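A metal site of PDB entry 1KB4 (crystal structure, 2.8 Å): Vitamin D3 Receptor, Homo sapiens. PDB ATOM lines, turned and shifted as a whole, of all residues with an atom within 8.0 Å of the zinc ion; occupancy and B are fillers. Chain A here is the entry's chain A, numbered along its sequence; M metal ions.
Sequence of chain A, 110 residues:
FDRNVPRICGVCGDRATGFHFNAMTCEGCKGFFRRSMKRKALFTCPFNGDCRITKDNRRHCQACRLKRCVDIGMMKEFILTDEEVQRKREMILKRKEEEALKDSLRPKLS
The side-chain sulfur (SG) of Cys 64 lies close to the backbone NH (N) of Asp 50, at 3.7 Å.
SG of Cys 45 lies close to N of Gly 49 (3.3 Å).
The backbone NH of Phe 47 sits close to the side-chain sulfur of Cys 45, at 3.4 Å.
The zinc ion is bound by the side-chain sulfur (SG) of Cys 64, at 2.2 Å.
The side-chain sulfur (SG) of Cys 61 binds the zinc ion, 2.2 Å away.
The zinc ion is bound by SG of Cys 45 (2.3 Å).
The side-chain sulfur (SG) of Cys 51 is bound to the zinc ion (2.4 Å).
Of the 18 residues printed, 4 come within 4 Å of the zinc ion.
The nearest printed residue that does not touch the zinc ion is Gly 49 (4.3 Å).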
ATOM      1  N   THR A  44     -27.332  19.136  18.576  1.00  0.00           N
ATOM      2  CA  THR A  44     -26.041  18.985  19.204  1.00  0.00           C
ATOM      3  C   THR A  44     -26.235  18.150  20.458  1.00  0.00           C
ATOM      4  O   THR A  44     -27.057  18.488  21.303  1.00  0.00           O
ATOM      5  CB  THR A  44     -25.357  20.351  19.590  1.00  0.00           C
ATOM      6  OG1 THR A  44     -25.298  20.469  21.025  1.00  0.00           O
ATOM      7  CG2 THR A  44     -26.108  21.561  18.974  1.00  0.00           C
ATOM      8  N   CYS A  45     -25.489  17.045  20.555  1.00  0.00           N
ATOM      9  CA  CYS A  45     -25.543  16.113  21.673  1.00  0.00           C
ATOM     10  C   CYS A  45     -25.170  16.662  23.071  1.00  0.00           C
ATOM     11  O   CYS A  45     -24.123  17.247  23.262  1.00  0.00           O
ATOM     12  CB  CYS A  45     -24.656  14.950  21.321  1.00  0.00           C
ATOM     13  SG  CYS A  45     -24.721  13.652  22.450  1.00  0.00           S
ATOM     14  N   PRO A  46     -26.032  16.488  24.083  1.00  0.00           N
ATOM     15  CA  PRO A  46     -25.596  17.025  25.367  1.00  0.00           C
ATOM     16  C   PRO A  46     -24.619  16.107  26.126  1.00  0.00           C
ATOM     17  O   PRO A  46     -24.110  16.455  27.206  1.00  0.00           O
ATOM     18  CB  PRO A  46     -26.921  17.234  26.111  1.00  0.00           C
ATOM     19  CG  PRO A  46     -27.735  16.138  25.641  1.00  0.00           C
ATOM     20  CD  PRO A  46     -27.462  16.149  24.127  1.00  0.00           C
ATOM     21  N   PHE A  47     -24.353  14.943  25.551  1.00  0.00           N
ATOM     22  CA  PHE A  47     -23.449  13.982  26.164  1.00  0.00           C
ATOM     23  C   PHE A  47     -22.070  13.900  25.514  1.00  0.00           C
ATOM     24  O   PHE A  47     -21.357  14.888  25.475  1.00  0.00           O
ATOM     25  CB  PHE A  47     -24.122  12.620  26.192  1.00  0.00           C
ATOM     26  CG  PHE A  47     -25.466  12.663  26.818  1.00  0.00           C
ATOM     27  CD1 PHE A  47     -25.608  12.726  28.181  1.00  0.00           C
ATOM     28  CD2 PHE A  47     -26.607  12.735  26.018  1.00  0.00           C
ATOM     29  CE1 PHE A  47     -26.869  12.863  28.753  1.00  0.00           C
ATOM     30  CE2 PHE A  47     -27.871  12.874  26.577  1.00  0.00           C
ATOM     31  CZ  PHE A  47     -28.004  12.940  27.938  1.00  0.00           C
ATOM     32  N   ASN A  48     -21.706  12.737  25.003  1.00  0.00           N
ATOM     33  CA  ASN A  48     -20.384  12.580  24.404  1.00  0.00           C
ATOM     34  C   ASN A  48     -20.433  12.373  22.919  1.00  0.00           C
ATOM     35  O   ASN A  48     -19.389  12.170  22.284  1.00  0.00           O
ATOM     36  CB  ASN A  48     -19.657  11.429  25.068  1.00  0.00           C
ATOM     37  CG  ASN A  48     -19.775  11.463  26.567  1.00  0.00           C
ATOM     38  OD1 ASN A  48     -19.351  12.421  27.233  1.00  0.00           O
ATOM     39  ND2 ASN A  48     -20.370  10.415  27.114  1.00  0.00           N
ATOM     40  N   GLY A  49     -21.644  12.431  22.372  1.00  0.00           N
ATOM     41  CA  GLY A  49     -21.846  12.308  20.949  1.00  0.00           C
ATOM     42  C   GLY A  49     -21.796  10.892  20.467  1.00  0.00           C
ATOM     43  O   GLY A  49     -21.415  10.623  19.330  1.00  0.00           O
ATOM     44  N   ASP A  50     -22.164   9.966  21.338  1.00  0.00           N
ATOM     45  CA  ASP A  50     -22.219   8.578  20.938  1.00  0.00           C
ATOM     46  C   ASP A  50     -23.232   7.810  21.735  1.00  0.00           C
ATOM     47  O   ASP A  50     -22.975   6.655  22.144  1.00  0.00           O
ATOM     48  CB  ASP A  50     -20.875   7.898  21.045  1.00  0.00           C
ATOM     49  CG  ASP A  50     -20.260   8.048  22.377  1.00  0.00           C
ATOM     50  OD1 ASP A  50     -20.950   8.330  23.394  1.00  0.00           O
ATOM     51  OD2 ASP A  50     -19.055   7.873  22.405  1.00  0.00           O
ATOM     52  N   CYS A  51     -24.367   8.455  21.947  1.00  0.00           N
ATOM     53  CA  CYS A  51     -25.465   7.849  22.656  1.00  0.00           C
ATOM     54  C   CYS A  51     -25.887   6.544  21.987  1.00  0.00           C
ATOM     55  O   CYS A  51     -25.619   6.313  20.797  1.00  0.00           O
ATOM     56  CB  CYS A  51     -26.635   8.812  22.689  1.00  0.00           C
ATOM     57  SG  CYS A  51     -26.283  10.431  23.410  1.00  0.00           S
ATOM     58  N   ARG A  52     -26.517   5.672  22.756  1.00  0.00           N
ATOM     59  CA  ARG A  52     -26.982   4.390  22.206  1.00  0.00           C
ATOM     60  C   ARG A  52     -28.492   4.546  22.042  1.00  0.00           C
ATOM     61  O   ARG A  52     -29.249   4.486  23.021  1.00  0.00           O
ATOM     62  CB  ARG A  52     -26.639   3.213  23.160  1.00  0.00           C
ATOM     63  CG  ARG A  52     -25.158   3.054  23.435  1.00  0.00           C
ATOM     64  CD  ARG A  52     -24.844   1.662  23.707  1.00  0.00           C
ATOM     65  NE  ARG A  52     -23.412   1.438  23.824  1.00  0.00           N
ATOM     66  CZ  ARG A  52     -22.870   0.313  24.280  1.00  0.00           C
ATOM     67  NH1 ARG A  52     -23.657  -0.689  24.653  1.00  0.00           N
ATOM     68  NH2 ARG A  52     -21.542   0.174  24.336  1.00  0.00           N
ATOM     69  N   ILE A  53     -28.931   4.784  20.818  1.00  0.00           N
ATOM     70  CA  ILE A  53     -30.336   5.024  20.594  1.00  0.00           C
ATOM     71  C   ILE A  53     -31.071   3.750  20.877  1.00  0.00           C
ATOM     72  O   ILE A  53     -30.620   2.683  20.491  1.00  0.00           O
ATOM     73  CB  ILE A  53     -30.614   5.488  19.130  1.00  0.00           C
ATOM     74  CG1 ILE A  53     -29.616   6.559  18.688  1.00  0.00           C
ATOM     75  CG2 ILE A  53     -31.998   6.072  19.029  1.00  0.00           C
ATOM     76  CD1 ILE A  53     -29.504   7.693  19.653  1.00  0.00           C
ATOM     77  N   ASN A  57     -35.452   5.861  24.430  1.00  0.00           N
ATOM     78  CA  ASN A  57     -34.666   7.029  24.796  1.00  0.00           C
ATOM     79  C   ASN A  57     -34.328   7.808  23.568  1.00  0.00           C
ATOM     80  O   ASN A  57     -33.652   8.819  23.685  1.00  0.00           O
ATOM     81  CB  ASN A  57     -33.360   6.633  25.437  1.00  0.00           C
ATOM     82  CG  ASN A  57     -32.380   6.134  24.424  1.00  0.00           C
ATOM     83  OD1 ASN A  57     -32.744   5.397  23.527  1.00  0.00           O
ATOM     84  ND2 ASN A  57     -31.125   6.533  24.555  1.00  0.00           N
ATOM     85  N   HIS A  60     -34.531  11.447  23.423  1.00  0.00           N
ATOM     86  CA  HIS A  60     -33.547  12.229  24.181  1.00  0.00           C
ATOM     87  C   HIS A  60     -32.285  12.749  23.458  1.00  0.00           C
ATOM     88  O   HIS A  60     -31.652  13.672  23.932  1.00  0.00           O
ATOM     89  CB  HIS A  60     -33.058  11.445  25.409  1.00  0.00           C
ATOM     90  CG  HIS A  60     -34.156  10.985  26.333  1.00  0.00           C
ATOM     91  ND1 HIS A  60     -35.207  11.799  26.729  1.00  0.00           N
ATOM     92  CD2 HIS A  60     -34.312   9.802  26.988  1.00  0.00           C
ATOM     93  CE1 HIS A  60     -35.970  11.128  27.579  1.00  0.00           C
ATOM     94  NE2 HIS A  60     -35.445   9.921  27.755  1.00  0.00           N
ATOM     95  N   CYS A  61     -31.881  12.133  22.365  1.00  0.00           N
ATOM     96  CA  CYS A  61     -30.771  12.707  21.676  1.00  0.00           C
ATOM     97  C   CYS A  61     -31.002  12.773  20.158  1.00  0.00           C
ATOM     98  O   CYS A  61     -30.603  11.843  19.411  1.00  0.00           O
ATOM     99  CB  CYS A  61     -29.482  11.985  21.981  1.00  0.00           C
ATOM    100  SG  CYS A  61     -28.074  13.002  21.441  1.00  0.00           S
ATOM    101  N   GLN A  62     -31.628  13.870  19.726  1.00  0.00           N
ATOM    102  CA  GLN A  62     -31.921  14.082  18.319  1.00  0.00           C
ATOM    103  C   GLN A  62     -30.664  14.103  17.490  1.00  0.00           C
ATOM    104  O   GLN A  62     -30.655  13.589  16.367  1.00  0.00           O
ATOM    105  CB  GLN A  62     -32.650  15.370  18.151  1.00  0.00           C
ATOM    106  CG  GLN A  62     -33.595  15.581  19.276  1.00  0.00           C
ATOM    107  CD  GLN A  62     -34.285  16.938  19.217  1.00  0.00           C
ATOM    108  OE1 GLN A  62     -33.698  18.002  19.566  1.00  0.00           O
ATOM    109  NE2 GLN A  62     -35.511  16.917  18.768  1.00  0.00           N
ATOM    110  N   ALA A  63     -29.605  14.662  18.066  1.00  0.00           N
ATOM    111  CA  ALA A  63     -28.282  14.756  17.435  1.00  0.00           C
ATOM    112  C   ALA A  63     -27.817  13.393  17.000  1.00  0.00           C
ATOM    113  O   ALA A  63     -27.577  13.166  15.833  1.00  0.00           O
ATOM    114  CB  ALA A  63     -27.305  15.321  18.382  1.00  0.00           C
ATOM    115  N   CYS A  64     -27.739  12.465  17.952  1.00  0.00           N
ATOM    116  CA  CYS A  64     -27.304  11.108  17.682  1.00  0.00           C
ATOM    117  C   CYS A  64     -28.290  10.304  16.891  1.00  0.00           C
ATOM    118  O   CYS A  64     -27.899   9.492  16.080  1.00  0.00           O
ATOM    119  CB  CYS A  64     -26.969  10.382  18.989  1.00  0.00           C
ATOM    120  SG  CYS A  64     -25.421  10.933  19.850  1.00  0.00           S
ATOM    121  N   ARG A  65     -29.591  10.501  17.129  1.00  0.00           N
ATOM    122  CA  ARG A  65     -30.611   9.775  16.361  1.00  0.00           C
ATOM    123  C   ARG A  65     -30.434  10.051  14.872  1.00  0.00           C
ATOM    124  O   ARG A  65     -30.293   9.122  14.093  1.00  0.00           O
ATOM    125  CB  ARG A  65     -31.989  10.208  16.785  1.00  0.00           C
ATOM    126  CG  ARG A  65     -33.124   9.310  16.338  1.00  0.00           C
ATOM    127  CD  ARG A  65     -34.406   9.851  16.841  1.00  0.00           C
ATOM    128  NE  ARG A  65     -35.544   9.000  16.530  1.00  0.00           N
ATOM    129  CZ  ARG A  65     -36.813   9.260  16.892  1.00  0.00           C
ATOM    130  NH1 ARG A  65     -37.100  10.347  17.591  1.00  0.00           N
ATOM    131  NH2 ARG A  65     -37.773   8.431  16.557  1.00  0.00           N
ATOM    132  N   LYS A  67     -27.945  11.393  13.281  1.00  0.00           N
ATOM    133  CA  LYS A  67     -26.659  10.953  12.760  1.00  0.00           C
ATOM    134  C   LYS A  67     -26.716   9.459  12.488  1.00  0.00           C
ATOM    135  O   LYS A  67     -26.144   8.960  11.525  1.00  0.00           O
ATOM    136  CB  LYS A  67     -25.555  11.265  13.743  1.00  0.00           C
ATOM    137  CG  LYS A  67     -24.213  11.200  13.083  1.00  0.00           C
ATOM    138  CD  LYS A  67     -23.041  11.027  14.077  1.00  0.00           C
ATOM    139  CE  LYS A  67     -21.755  10.779  13.253  1.00  0.00           C
ATOM    140  NZ  LYS A  67     -22.007   9.941  11.974  1.00  0.00           N
HETATM  141 ZN    ZN M   1     -26.109  12.002  21.633  1.00  0.00          ZN
